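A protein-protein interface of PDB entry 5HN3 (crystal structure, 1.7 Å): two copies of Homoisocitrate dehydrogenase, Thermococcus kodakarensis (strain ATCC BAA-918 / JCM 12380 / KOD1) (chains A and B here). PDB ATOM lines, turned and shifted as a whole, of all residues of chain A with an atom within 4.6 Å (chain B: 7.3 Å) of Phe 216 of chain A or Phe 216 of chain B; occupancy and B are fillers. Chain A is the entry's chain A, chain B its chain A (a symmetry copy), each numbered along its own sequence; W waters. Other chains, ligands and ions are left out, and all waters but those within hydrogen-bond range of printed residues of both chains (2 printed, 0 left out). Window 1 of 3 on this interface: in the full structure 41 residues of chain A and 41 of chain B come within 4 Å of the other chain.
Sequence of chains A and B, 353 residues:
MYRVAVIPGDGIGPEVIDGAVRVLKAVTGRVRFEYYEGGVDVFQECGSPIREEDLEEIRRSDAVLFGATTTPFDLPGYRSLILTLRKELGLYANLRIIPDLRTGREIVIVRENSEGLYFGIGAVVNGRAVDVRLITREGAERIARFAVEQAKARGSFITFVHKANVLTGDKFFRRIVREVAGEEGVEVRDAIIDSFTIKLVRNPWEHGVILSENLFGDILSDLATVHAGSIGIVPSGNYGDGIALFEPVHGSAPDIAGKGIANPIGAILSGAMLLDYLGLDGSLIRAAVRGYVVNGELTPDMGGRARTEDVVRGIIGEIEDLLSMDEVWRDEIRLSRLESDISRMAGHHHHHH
NZ of Lys 163 of chain A sits at hydrogen-bond distance from O of Leu 215 of chain B (2.9 Å).
NZ of Lys 163 of chain B is in hydrogen-bond range of O of Leu 215 of chain A (2.9 Å).
The side-chain carboxylate (OE1) of Glu 112 of chain B is in hydrogen-bond range of the backbone NH (N) of Asn 214 of chain B (2.7 Å).
The backbone carbonyl oxygen of His 162 of chain B lies within hydrogen-bond range of the backbone NH of Ile 193 of chain B (2.8 Å).
The backbone NH (N) of Lys 163 of chain B is in hydrogen-bond range of the side-chain carboxylate (OD2) of Asp 170 of chain B (3.0 Å).
Among the printed residues, merely in contact across the chains: Asp 218 of chain A with Asp 194 of chain B (3.3 Å), Ile 219 of chain A with Asp 194 of chain B (3.5 Å), Ile 193 of chain A with Ile 219 of chain B (3.7 Å), Ile 219 of chain A with Ile 193 of chain B (3.7 Å), Lys 163 of chain A with Asn 214 of chain B (3.7 Å), Asn 214 of chain A with Lys 163 of chain B (3.7 Å), Phe 216 of chain A with Phe 216 of chain B (3.9 Å), Ile 219 of chain A with Ile 219 of chain B (3.9 Å) and Leu 215 of chain A with Val 166 of chain B (3.9 Å).
Printed residues of chain B within 4 Å of Phe 216 of chain A: Phe 216 (3.9 Å).
Phe 216 of chain B touches one residue of chain A.
Of the printed residues of chain B, Ile 219 of chain A touches Ile 193 (3.7 Å), Asp 194 (3.5 Å) and Ile 219 (3.9 Å).
Of the printed residues of chain A, Ile 219 of chain B touches Ile 193 (3.7 Å) and Ile 219 (3.9 Å).
Of the printed residues of chain B, Leu 215 of chain A touches Lys 163 and Val 166.
The nearest residue of chain A that does not touch Phe 216 of chain B is Leu 215 of chain A (4.1 Å).
The nearest printed residue of chain B that does not touch Asn 214 of chain A is Asp 194 of chain B (5.4 Å).
Of the 13 printed residues of chain A, 7 touch a printed residue of chain B.
Printed residues of chain A that touch a printed residue of chain B: Lys 163, Ile 193, Asn 214, Leu 215, Phe 216, Asp 218 and Ile 219.
Along chain A the printed residues that touch a printed residue of chain B span positions 163 to 219.
Among the printed residues, no Asp or Glu carboxylate lies within 4 Å of a Lys or Arg side-chain nitrogen of the other chain.
Ile 193 of chain A touches Ile 219 of chain B, and with the chains exchanged Ile 219 of chain A touches Ile 193 of chain B.
Phe 216 of chain B touches its own counterpart, Phe 216 of chain A.
Ile 219 of chain A touches its own counterpart, Ile 219 of chain B.
Of the 11 pairs that touch across the chains among the printed residues, 8 have their exchanged pair printed and touching as well.
Water W1 lies within hydrogen-bond range of the side-chain carboxylate (OD2) of Asp 218 of chain A, the side-chain amino group (NZ) of Lys 163 of chain B and the backbone carbonyl oxygen (O) of Asn 214 of chain A.
Water W2 lies within hydrogen-bond range of the side-chain carboxylate of Asp 218 of chain B, the side-chain amino group of Lys 163 of chain A and the backbone carbonyl oxygen of Asn 214 of chain B.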
ATOM      1  N   LYS A 163     -19.603  13.261  26.832  1.00  0.00           N
ATOM      2  CA  LYS A 163     -20.046  13.002  25.502  1.00  0.00           C
ATOM      3  C   LYS A 163     -20.984  14.153  24.993  1.00  0.00           C
ATOM      4  O   LYS A 163     -22.072  13.848  24.478  1.00  0.00           O
ATOM      5  CB  LYS A 163     -20.818  11.702  25.549  1.00  0.00           C
ATOM      6  CG  LYS A 163     -20.916  10.954  24.275  1.00  0.00           C
ATOM      7  CD  LYS A 163     -19.990   9.715  24.229  1.00  0.00           C
ATOM      8  CE  LYS A 163     -19.944   9.320  22.768  1.00  0.00           C
ATOM      9  NZ  LYS A 163     -19.291   8.036  22.461  1.00  0.00           N
ATOM     10  N   LEU A 167     -24.731  14.123  23.558  1.00  0.00           N
ATOM     11  CA  LEU A 167     -25.753  14.312  24.589  1.00  0.00           C
ATOM     12  C   LEU A 167     -25.784  15.757  25.036  1.00  0.00           C
ATOM     13  O   LEU A 167     -24.818  16.350  25.514  1.00  0.00           O
ATOM     14  CB  LEU A 167     -25.551  13.355  25.775  1.00  0.00           C
ATOM     15  CG  LEU A 167     -25.617  11.871  25.462  1.00  0.00           C
ATOM     16  CD1 LEU A 167     -25.190  11.073  26.673  1.00  0.00           C
ATOM     17  CD2 LEU A 167     -26.993  11.409  24.998  1.00  0.00           C
ATOM     18  N   ASP A 170     -24.797  16.523  28.630  1.00  0.00           N
ATOM     19  CA  ASP A 170     -23.359  16.710  28.836  1.00  0.00           C
ATOM     20  C   ASP A 170     -22.842  18.057  28.451  1.00  0.00           C
ATOM     21  O   ASP A 170     -21.950  18.587  29.089  1.00  0.00           O
ATOM     22  CB  ASP A 170     -22.578  15.636  28.051  1.00  0.00           C
ATOM     23  CG  ASP A 170     -22.626  14.280  28.728  1.00  0.00           C
ATOM     24  OD1 ASP A 170     -23.722  13.710  28.916  1.00  0.00           O
ATOM     25  OD2 ASP A 170     -21.542  13.730  29.046  1.00  0.00           O
ATOM     26  N   ILE A 193     -15.018  11.412  26.171  1.00  0.00           N
ATOM     27  CA  ILE A 193     -14.617  10.111  26.796  1.00  0.00           C
ATOM     28  C   ILE A 193     -13.883   9.144  25.834  1.00  0.00           C
ATOM     29  O   ILE A 193     -12.861   8.547  26.221  1.00  0.00           O
ATOM     30  CB  ILE A 193     -15.752   9.367  27.522  1.00  0.00           C
ATOM     31  CG1 ILE A 193     -15.147   8.132  28.253  1.00  0.00           C
ATOM     32  CG2 ILE A 193     -16.909   9.007  26.598  1.00  0.00           C
ATOM     33  CD1 ILE A 193     -15.919   7.631  29.418  1.00  0.00           C
ATOM     34  N   SER A 212     -16.892  13.560  35.721  1.00  0.00           N
ATOM     35  CA  SER A 212     -17.736  13.021  34.653  1.00  0.00           C
ATOM     36  C   SER A 212     -19.040  12.523  35.265  1.00  0.00           C
ATOM     37  O   SER A 212     -19.029  11.788  36.282  1.00  0.00           O
ATOM     38  CB  SER A 212     -16.954  11.867  33.955  1.00  0.00           C
ATOM     39  OG  SER A 212     -17.545  11.313  32.787  1.00  0.00           O
ATOM     40  N   GLU A 213     -20.177  12.861  34.642  1.00  0.00           N
ATOM     41  CA  GLU A 213     -21.411  12.209  35.055  1.00  0.00           C
ATOM     42  C   GLU A 213     -21.255  10.707  35.059  1.00  0.00           C
ATOM     43  O   GLU A 213     -20.557  10.140  34.180  1.00  0.00           O
ATOM     44  CB  GLU A 213     -22.596  12.626  34.192  1.00  0.00           C
ATOM     45  CG  GLU A 213     -22.639  11.957  32.835  1.00  0.00           C
ATOM     46  CD  GLU A 213     -23.276  12.786  31.763  1.00  0.00           C
ATOM     47  OE1 GLU A 213     -23.247  14.067  31.850  1.00  0.00           O
ATOM     48  OE2 GLU A 213     -23.794  12.122  30.848  1.00  0.00           O
ATOM     49  N   ASN A 214     -21.920  10.032  35.985  1.00  0.00           N
ATOM     50  CA  ASN A 214     -21.612   8.615  36.213  1.00  0.00           C
ATOM     51  C   ASN A 214     -21.848   7.648  35.067  1.00  0.00           C
ATOM     52  O   ASN A 214     -21.176   6.612  35.004  1.00  0.00           O
ATOM     53  CB  ASN A 214     -22.173   8.089  37.546  1.00  0.00           C
ATOM     54  CG  ASN A 214     -23.673   7.925  37.543  1.00  0.00           C
ATOM     55  OD1 ASN A 214     -24.281   7.568  36.541  1.00  0.00           O
ATOM     56  ND2 ASN A 214     -24.271   8.136  38.695  1.00  0.00           N
ATOM     57  N   LEU A 215     -22.733   7.982  34.116  1.00  0.00           N
ATOM     58  CA  LEU A 215     -22.932   7.169  32.965  1.00  0.00           C
ATOM     59  C   LEU A 215     -21.596   6.878  32.231  1.00  0.00           C
ATOM     60  O   LEU A 215     -21.356   5.760  31.821  1.00  0.00           O
ATOM     61  CB  LEU A 215     -23.928   7.831  31.994  1.00  0.00           C
ATOM     62  CG  LEU A 215     -24.400   6.985  30.824  1.00  0.00           C
ATOM     63  CD1 LEU A 215     -25.255   5.774  31.231  1.00  0.00           C
ATOM     64  CD2 LEU A 215     -25.155   7.893  29.835  1.00  0.00           C
ATOM     65  N   PHE A 216     -20.736   7.870  32.224  1.00  0.00           N
ATOM     66  CA  PHE A 216     -19.370   7.771  31.610  1.00  0.00           C
ATOM     67  C   PHE A 216     -18.349   7.707  32.734  1.00  0.00           C
ATOM     68  O   PHE A 216     -17.352   7.022  32.604  1.00  0.00           O
ATOM     69  CB  PHE A 216     -19.081   8.966  30.710  1.00  0.00           C
ATOM     70  CG  PHE A 216     -20.067   9.052  29.567  1.00  0.00           C
ATOM     71  CD1 PHE A 216     -20.218   7.985  28.727  1.00  0.00           C
ATOM     72  CD2 PHE A 216     -20.954  10.098  29.473  1.00  0.00           C
ATOM     73  CE1 PHE A 216     -21.148   7.957  27.687  1.00  0.00           C
ATOM     74  CE2 PHE A 216     -21.921  10.076  28.456  1.00  0.00           C
ATOM     75  CZ  PHE A 216     -22.053   9.014  27.601  1.00  0.00           C
ATOM     76  N   GLY A 217     -18.566   8.442  33.814  1.00  0.00           N
ATOM     77  CA  GLY A 217     -17.554   8.493  34.872  1.00  0.00           C
ATOM     78  C   GLY A 217     -17.326   7.182  35.567  1.00  0.00           C
ATOM     79  O   GLY A 217     -16.168   6.914  36.050  1.00  0.00           O
ATOM     80  N   ASP A 218     -18.341   6.334  35.664  1.00  0.00           N
ATOM     81  CA  ASP A 218     -18.169   5.006  36.268  1.00  0.00           C
ATOM     82  C   ASP A 218     -17.335   4.092  35.347  1.00  0.00           C
ATOM     83  O   ASP A 218     -16.693   3.154  35.843  1.00  0.00           O
ATOM     84  CB  ASP A 218     -19.439   4.349  36.614  1.00  0.00           C
ATOM     85  CG  ASP A 218     -20.169   5.050  37.784  1.00  0.00           C
ATOM     86  OD1 ASP A 218     -19.549   5.851  38.497  1.00  0.00           O
ATOM     87  OD2 ASP A 218     -21.339   4.728  37.966  1.00  0.00           O
ATOM     88  N   ILE A 219     -17.365   4.383  34.043  1.00  0.00           N
ATOM     89  CA  ILE A 219     -16.463   3.684  33.118  1.00  0.00           C
ATOM     90  C   ILE A 219     -15.061   4.069  33.545  1.00  0.00           C
ATOM     91  O   ILE A 219     -14.158   3.208  33.640  1.00  0.00           O
ATOM     92  CB  ILE A 219     -16.716   4.064  31.687  1.00  0.00           C
ATOM     93  CG1 ILE A 219     -18.182   3.792  31.339  1.00  0.00           C
ATOM     94  CG2 ILE A 219     -15.847   3.238  30.755  1.00  0.00           C
ATOM     95  CD1 ILE A 219     -18.554   4.200  29.921  1.00  0.00           C
ATOM     96  N   LEU A 220     -14.829   5.362  33.660  1.00  0.00           N
ATOM     97  CA  LEU A 220     -13.467   5.843  33.981  1.00  0.00           C
ATOM     98  C   LEU A 220     -12.989   5.318  35.301  1.00  0.00           C
ATOM     99  O   LEU A 220     -11.799   4.960  35.479  1.00  0.00           O
ATOM    100  CB  LEU A 220     -13.405   7.361  34.004  1.00  0.00           C
ATOM    101  CG  LEU A 220     -13.766   8.024  32.675  1.00  0.00           C
ATOM    102  CD1 LEU A 220     -13.730   9.528  32.787  1.00  0.00           C
ATOM    103  CD2 LEU A 220     -12.884   7.618  31.523  1.00  0.00           C
ATOM    104  N   ILE B 109     -14.609  -4.700  16.600  1.00  0.00           N
ATOM    105  CA  ILE B 109     -15.595  -3.859  17.270  1.00  0.00           C
ATOM    106  C   ILE B 109     -16.616  -3.353  16.255  1.00  0.00           C
ATOM    107  O   ILE B 109     -16.315  -2.525  15.391  1.00  0.00           O
ATOM    108  CB  ILE B 109     -14.983  -2.662  18.002  1.00  0.00           C
ATOM    109  CG1 ILE B 109     -13.767  -3.082  18.819  1.00  0.00           C
ATOM    110  CG2 ILE B 109     -16.029  -1.993  18.931  1.00  0.00           C
ATOM    111  CD1 ILE B 109     -12.426  -2.690  18.176  1.00  0.00           C
ATOM    112  N   ARG B 111     -20.132  -1.258  15.730  1.00  0.00           N
ATOM    113  CA  ARG B 111     -21.091  -0.262  16.229  1.00  0.00           C
ATOM    114  C   ARG B 111     -21.892   0.207  15.021  1.00  0.00           C
ATOM    115  O   ARG B 111     -21.462   0.034  13.882  1.00  0.00           O
ATOM    116  CB  ARG B 111     -20.437   0.966  16.859  1.00  0.00           C
ATOM    117  CG  ARG B 111     -19.369   0.728  17.891  1.00  0.00           C
ATOM    118  CD  ARG B 111     -18.007   0.486  17.285  1.00  0.00           C
ATOM    119  NE  ARG B 111     -17.398   1.682  16.707  1.00  0.00           N
ATOM    120  CZ  ARG B 111     -16.774   1.685  15.539  1.00  0.00           C
ATOM    121  NH1 ARG B 111     -16.254   2.804  15.094  1.00  0.00           N
ATOM    122  NH2 ARG B 111     -16.669   0.564  14.811  1.00  0.00           N
ATOM    123  N   GLU B 112     -23.010   0.878  15.276  1.00  0.00           N
ATOM    124  CA  GLU B 112     -23.693   1.592  14.190  1.00  0.00           C
ATOM    125  C   GLU B 112     -22.989   2.880  13.846  1.00  0.00           C
ATOM    126  O   GLU B 112     -22.425   3.561  14.709  1.00  0.00           O
ATOM    127  CB  GLU B 112     -25.180   1.831  14.541  1.00  0.00           C
ATOM    128  CG  GLU B 112     -25.540   3.021  15.383  1.00  0.00           C
ATOM    129  CD  GLU B 112     -25.297   2.868  16.891  1.00  0.00           C
ATOM    130  OE1 GLU B 112     -24.514   1.978  17.280  1.00  0.00           O
ATOM    131  OE2 GLU B 112     -25.951   3.612  17.655  1.00  0.00           O
ATOM    132  N   TYR B 118     -30.204   4.659  16.917  1.00  0.00           N
ATOM    133  CA  TYR B 118     -30.939   5.479  17.843  1.00  0.00           C
ATOM    134  C   TYR B 118     -31.351   6.781  17.204  1.00  0.00           C
ATOM    135  O   TYR B 118     -30.663   7.321  16.354  1.00  0.00           O
ATOM    136  CB  TYR B 118     -30.102   5.809  19.101  1.00  0.00           C
ATOM    137  CG  TYR B 118     -30.040   4.703  20.124  1.00  0.00           C
ATOM    138  CD1 TYR B 118     -29.043   3.713  20.079  1.00  0.00           C
ATOM    139  CD2 TYR B 118     -30.987   4.618  21.139  1.00  0.00           C
ATOM    140  CE1 TYR B 118     -28.997   2.683  21.017  1.00  0.00           C
ATOM    141  CE2 TYR B 118     -30.921   3.603  22.090  1.00  0.00           C
ATOM    142  CZ  TYR B 118     -29.918   2.639  22.037  1.00  0.00           C
ATOM    143  OH  TYR B 118     -29.878   1.632  22.982  1.00  0.00           O
ATOM    144  N   VAL B 161     -21.622  -5.469  24.623  1.00  0.00           N
ATOM    145  CA  VAL B 161     -21.171  -4.567  25.695  1.00  0.00           C
ATOM    146  C   VAL B 161     -22.114  -3.366  25.753  1.00  0.00           C
ATOM    147  O   VAL B 161     -22.472  -2.784  24.727  1.00  0.00           O
ATOM    148  CB  VAL B 161     -19.701  -4.158  25.464  1.00  0.00           C
ATOM    149  CG1 VAL B 161     -19.194  -3.372  26.655  1.00  0.00           C
ATOM    150  CG2 VAL B 161     -18.909  -5.420  25.223  1.00  0.00           C
ATOM    151  N   HIS B 162     -22.501  -2.988  26.962  1.00  0.00           N
ATOM    152  CA  HIS B 162     -23.671  -2.157  27.149  1.00  0.00           C
ATOM    153  C   HIS B 162     -23.731  -1.499  28.526  1.00  0.00           C
ATOM    154  O   HIS B 162     -22.859  -1.673  29.401  1.00  0.00           O
ATOM    155  CB  HIS B 162     -24.883  -3.094  26.960  1.00  0.00           C
ATOM    156  CG  HIS B 162     -24.996  -4.091  28.054  1.00  0.00           C
ATOM    157  ND1 HIS B 162     -24.631  -5.409  27.923  1.00  0.00           N
ATOM    158  CD2 HIS B 162     -25.357  -3.944  29.349  1.00  0.00           C
ATOM    159  CE1 HIS B 162     -24.762  -6.023  29.080  1.00  0.00           C
ATOM    160  NE2 HIS B 162     -25.259  -5.167  29.939  1.00  0.00           N
ATOM    161  N   LYS B 163     -24.798  -0.717  28.724  1.00  0.00           N
ATOM    162  CA  LYS B 163     -25.163  -0.167  29.988  1.00  0.00           C
ATOM    163  C   LYS B 163     -26.680  -0.433  30.293  1.00  0.00           C
ATOM    164  O   LYS B 163     -27.388   0.519  30.660  1.00  0.00           O
ATOM    165  CB  LYS B 163     -24.919   1.323  29.896  1.00  0.00           C
ATOM    166  CG  LYS B 163     -24.704   2.029  31.181  1.00  0.00           C
ATOM    167  CD  LYS B 163     -23.222   2.400  31.426  1.00  0.00           C
ATOM    168  CE  LYS B 163     -23.149   2.752  32.896  1.00  0.00           C
ATOM    169  NZ  LYS B 163     -21.883   3.344  33.362  1.00  0.00           N
ATOM    170  N   ALA B 164     -27.058  -1.679  30.146  1.00  0.00           N
ATOM    171  CA  ALA B 164     -28.457  -2.199  30.352  1.00  0.00           C
ATOM    172  C   ALA B 164     -28.903  -2.048  31.771  1.00  0.00           C
ATOM    173  O   ALA B 164     -30.125  -2.064  32.071  1.00  0.00           O
ATOM    174  CB  ALA B 164     -28.606  -3.624  29.895  1.00  0.00           C
ATOM    175  N   VAL B 166     -28.601   0.704  33.380  1.00  0.00           N
ATOM    176  CA  VAL B 166     -28.995   2.096  33.498  1.00  0.00           C
ATOM    177  C   VAL B 166     -29.971   2.486  32.392  1.00  0.00           C
ATOM    178  O   VAL B 166     -30.948   3.211  32.660  1.00  0.00           O
ATOM    179  CB  VAL B 166     -27.784   3.044  33.415  1.00  0.00           C
ATOM    180  CG1 VAL B 166     -28.200   4.499  33.499  1.00  0.00           C
ATOM    181  CG2 VAL B 166     -26.820   2.768  34.533  1.00  0.00           C
ATOM    182  N   LEU B 167     -29.715   2.041  31.167  1.00  0.00           N
ATOM    183  CA  LEU B 167     -30.461   2.490  29.990  1.00  0.00           C
ATOM    184  C   LEU B 167     -31.336   1.372  29.468  1.00  0.00           C
ATOM    185  O   LEU B 167     -30.909   0.276  29.106  1.00  0.00           O
ATOM    186  CB  LEU B 167     -29.528   3.038  28.898  1.00  0.00           C
ATOM    187  CG  LEU B 167     -28.683   4.241  29.275  1.00  0.00           C
ATOM    188  CD1 LEU B 167     -27.676   4.522  28.184  1.00  0.00           C
ATOM    189  CD2 LEU B 167     -29.502   5.494  29.558  1.00  0.00           C
ATOM    190  N   ASP B 170     -30.549  -0.034  26.021  1.00  0.00           N
ATOM    191  CA  ASP B 170     -29.546  -1.101  26.017  1.00  0.00           C
ATOM    192  C   ASP B 170     -30.063  -2.447  26.402  1.00  0.00           C
ATOM    193  O   ASP B 170     -29.629  -3.455  25.873  1.00  0.00           O
ATOM    194  CB  ASP B 170     -28.386  -0.726  26.963  1.00  0.00           C
ATOM    195  CG  ASP B 170     -27.464   0.314  26.358  1.00  0.00           C
ATOM    196  OD1 ASP B 170     -27.908   1.440  26.043  1.00  0.00           O
ATOM    197  OD2 ASP B 170     -26.246   0.034  26.230  1.00  0.00           O
ATOM    198  N   ILE B 193     -20.240  -2.164  30.141  1.00  0.00           N
ATOM    199  CA  ILE B 193     -19.020  -1.447  29.651  1.00  0.00           C
ATOM    200  C   ILE B 193     -17.989  -1.117  30.759  1.00  0.00           C
ATOM    201  O   ILE B 193     -16.778  -1.325  30.556  1.00  0.00           O
ATOM    202  CB  ILE B 193     -19.304  -0.192  28.807  1.00  0.00           C
ATOM    203  CG1 ILE B 193     -17.955   0.339  28.237  1.00  0.00           C
ATOM    204  CG2 ILE B 193     -20.089   0.868  29.570  1.00  0.00           C
ATOM    205  CD1 ILE B 193     -18.054   1.154  27.000  1.00  0.00           C
ATOM    206  N   ASP B 194     -18.425  -0.647  31.942  1.00  0.00           N
ATOM    207  CA  ASP B 194     -17.549  -0.188  32.974  1.00  0.00           C
ATOM    208  C   ASP B 194     -16.428  -1.214  33.258  1.00  0.00           C
ATOM    209  O   ASP B 194     -15.262  -0.892  33.115  1.00  0.00           O
ATOM    210  CB  ASP B 194     -18.287   0.081  34.290  1.00  0.00           C
ATOM    211  CG  ASP B 194     -19.466   1.018  34.176  1.00  0.00           C
ATOM    212  OD1 ASP B 194     -19.910   1.346  33.061  1.00  0.00           O
ATOM    213  OD2 ASP B 194     -19.979   1.402  35.280  1.00  0.00           O
ATOM    214  N   SER B 212     -21.636  -3.134  20.321  1.00  0.00           N
ATOM    215  CA  SER B 212     -22.091  -2.126  21.281  1.00  0.00           C
ATOM    216  C   SER B 212     -22.676  -0.947  20.514  1.00  0.00           C
ATOM    217  O   SER B 212     -22.053  -0.440  19.548  1.00  0.00           O
ATOM    218  CB  SER B 212     -20.866  -1.695  22.145  1.00  0.00           C
ATOM    219  OG  SER B 212     -21.134  -0.832  23.243  1.00  0.00           O
ATOM    220  N   GLU B 213     -23.844  -0.454  20.945  1.00  0.00           N
ATOM    221  CA  GLU B 213     -24.308   0.810  20.392  1.00  0.00           C
ATOM    222  C   GLU B 213     -23.236   1.869  20.490  1.00  0.00           C
ATOM    223  O   GLU B 213     -22.474   1.910  21.490  1.00  0.00           O
ATOM    224  CB  GLU B 213     -25.597   1.285  21.051  1.00  0.00           C
ATOM    225  CG  GLU B 213     -25.403   1.899  22.420  1.00  0.00           C
ATOM    226  CD  GLU B 213     -26.568   1.720  23.344  1.00  0.00           C
ATOM    227  OE1 GLU B 213     -27.346   0.709  23.194  1.00  0.00           O
ATOM    228  OE2 GLU B 213     -26.674   2.609  24.206  1.00  0.00           O
ATOM    229  N   ASN B 214     -23.178   2.763  19.514  1.00  0.00           N
ATOM    230  CA  ASN B 214     -22.012   3.649  19.408  1.00  0.00           C
ATOM    231  C   ASN B 214     -21.744   4.605  20.556  1.00  0.00           C
ATOM    232  O   ASN B 214     -20.587   4.981  20.771  1.00  0.00           O
ATOM    233  CB  ASN B 214     -21.911   4.341  18.037  1.00  0.00           C
ATOM    234  CG  ASN B 214     -22.947   5.418  17.830  1.00  0.00           C
ATOM    235  OD1 ASN B 214     -23.327   6.132  18.750  1.00  0.00           O
ATOM    236  ND2 ASN B 214     -23.367   5.574  16.594  1.00  0.00           N
ATOM    237  N   LEU B 215     -22.767   4.958  21.350  1.00  0.00           N
ATOM    238  CA  LEU B 215     -22.570   5.772  22.501  1.00  0.00           C
ATOM    239  C   LEU B 215     -21.478   5.188  23.435  1.00  0.00           C
ATOM    240  O   LEU B 215     -20.647   5.919  23.933  1.00  0.00           O
ATOM    241  CB  LEU B 215     -23.888   5.944  23.280  1.00  0.00           C
ATOM    242  CG  LEU B 215     -23.880   6.957  24.411  1.00  0.00           C
ATOM    243  CD1 LEU B 215     -23.702   8.412  23.948  1.00  0.00           C
ATOM    244  CD2 LEU B 215     -25.173   6.788  25.231  1.00  0.00           C
ATOM    245  N   PHE B 216     -21.455   3.877  23.515  1.00  0.00           N
ATOM    246  CA  PHE B 216     -20.444   3.119  24.325  1.00  0.00           C
ATOM    247  C   PHE B 216     -19.465   2.463  23.367  1.00  0.00           C
ATOM    248  O   PHE B 216     -18.292   2.365  23.676  1.00  0.00           O
ATOM    249  CB  PHE B 216     -21.114   2.062  25.194  1.00  0.00           C
ATOM    250  CG  PHE B 216     -22.083   2.681  26.176  1.00  0.00           C
ATOM    251  CD1 PHE B 216     -21.643   3.643  27.039  1.00  0.00           C
ATOM    252  CD2 PHE B 216     -23.434   2.441  26.085  1.00  0.00           C
ATOM    253  CE1 PHE B 216     -22.483   4.309  27.932  1.00  0.00           C
ATOM    254  CE2 PHE B 216     -24.302   3.125  26.949  1.00  0.00           C
ATOM    255  CZ  PHE B 216     -23.854   4.072  27.831  1.00  0.00           C
ATOM    256  N   GLY B 217     -19.939   1.976  22.230  1.00  0.00           N
ATOM    257  CA  GLY B 217     -19.049   1.240  21.329  1.00  0.00           C
ATOM    258  C   GLY B 217     -17.943   2.070  20.744  1.00  0.00           C
ATOM    259  O   GLY B 217     -16.823   1.517  20.450  1.00  0.00           O
ATOM    260  N   ASP B 218     -18.162   3.363  20.545  1.00  0.00           N
ATOM    261  CA  ASP B 218     -17.102   4.246  20.044  1.00  0.00           C
ATOM    262  C   ASP B 218     -16.023   4.471  21.123  1.00  0.00           C
ATOM    263  O   ASP B 218     -14.868   4.761  20.775  1.00  0.00           O
ATOM    264  CB  ASP B 218     -17.599   5.541  19.551  1.00  0.00           C
ATOM    265  CG  ASP B 218     -18.427   5.402  18.252  1.00  0.00           C
ATOM    266  OD1 ASP B 218     -18.361   4.353  17.596  1.00  0.00           O
ATOM    267  OD2 ASP B 218     -19.085   6.382  17.919  1.00  0.00           O
ATOM    268  N   ILE B 219     -16.420   4.334  22.391  1.00  0.00           N
ATOM    269  CA  ILE B 219     -15.425   4.350  23.472  1.00  0.00           C
ATOM    270  C   ILE B 219     -14.543   3.141  23.235  1.00  0.00           C
ATOM    271  O   ILE B 219     -13.298   3.228  23.317  1.00  0.00           O
ATOM    272  CB  ILE B 219     -16.067   4.292  24.830  1.00  0.00           C
ATOM    273  CG1 ILE B 219     -17.058   5.450  24.975  1.00  0.00           C
ATOM    274  CG2 ILE B 219     -15.019   4.427  25.920  1.00  0.00           C
ATOM    275  CD1 ILE B 219     -17.805   5.445  26.300  1.00  0.00           C
ATOM    276  N   LEU B 220     -15.170   1.991  23.087  1.00  0.00           N
ATOM    277  CA  LEU B 220     -14.394   0.739  22.943  1.00  0.00           C
ATOM    278  C   LEU B 220     -13.506   0.771  21.735  1.00  0.00           C
ATOM    279  O   LEU B 220     -12.350   0.283  21.752  1.00  0.00           O
ATOM    280  CB  LEU B 220     -15.306  -0.472  22.850  1.00  0.00           C
ATOM    281  CG  LEU B 220     -16.194  -0.686  24.076  1.00  0.00           C
ATOM    282  CD1 LEU B 220     -17.105  -1.875  23.891  1.00  0.00           C
ATOM    283  CD2 LEU B 220     -15.435  -0.871  25.363  1.00  0.00           C
ATOM    284  N   SER B 221     -14.019   1.329  20.652  1.00  0.00           N
ATOM    285  CA  SER B 221     -13.258   1.274  19.389  1.00  0.00           C
ATOM    286  C   SER B 221     -12.006   2.149  19.474  1.00  0.00           C
ATOM    287  O   SER B 221     -10.961   1.794  18.845  1.00  0.00           O
ATOM    288  CB  SER B 221     -14.173   1.647  18.205  1.00  0.00           C
ATOM    289  OG  SER B 221     -14.530   2.961  18.285  1.00  0.00           O
ATOM    290  N   ASP B 222     -12.037   3.222  20.251  1.00  0.00           N
ATOM    291  CA  ASP B 222     -10.844   4.050  20.568  1.00  0.00           C
ATOM    292  C   ASP B 222      -9.991   3.403  21.630  1.00  0.00           C
ATOM    293  O   ASP B 222      -8.777   3.300  21.441  1.00  0.00           O
ATOM    294  CB  ASP B 222     -11.204   5.476  20.967  1.00  0.00           C
ATOM    295  CG  ASP B 222     -11.594   6.367  19.731  1.00  0.00           C
ATOM    296  OD1 ASP B 222     -11.307   5.964  18.594  1.00  0.00           O
ATOM    297  OD2 ASP B 222     -12.156   7.448  19.918  1.00  0.00           O
HETATM  298  O   HOH W   1     -22.918   3.927  35.894  1.00  0.00           O
HETATM  299  O   HOH W   2     -20.077   8.110  19.778  1.00  0.00           O
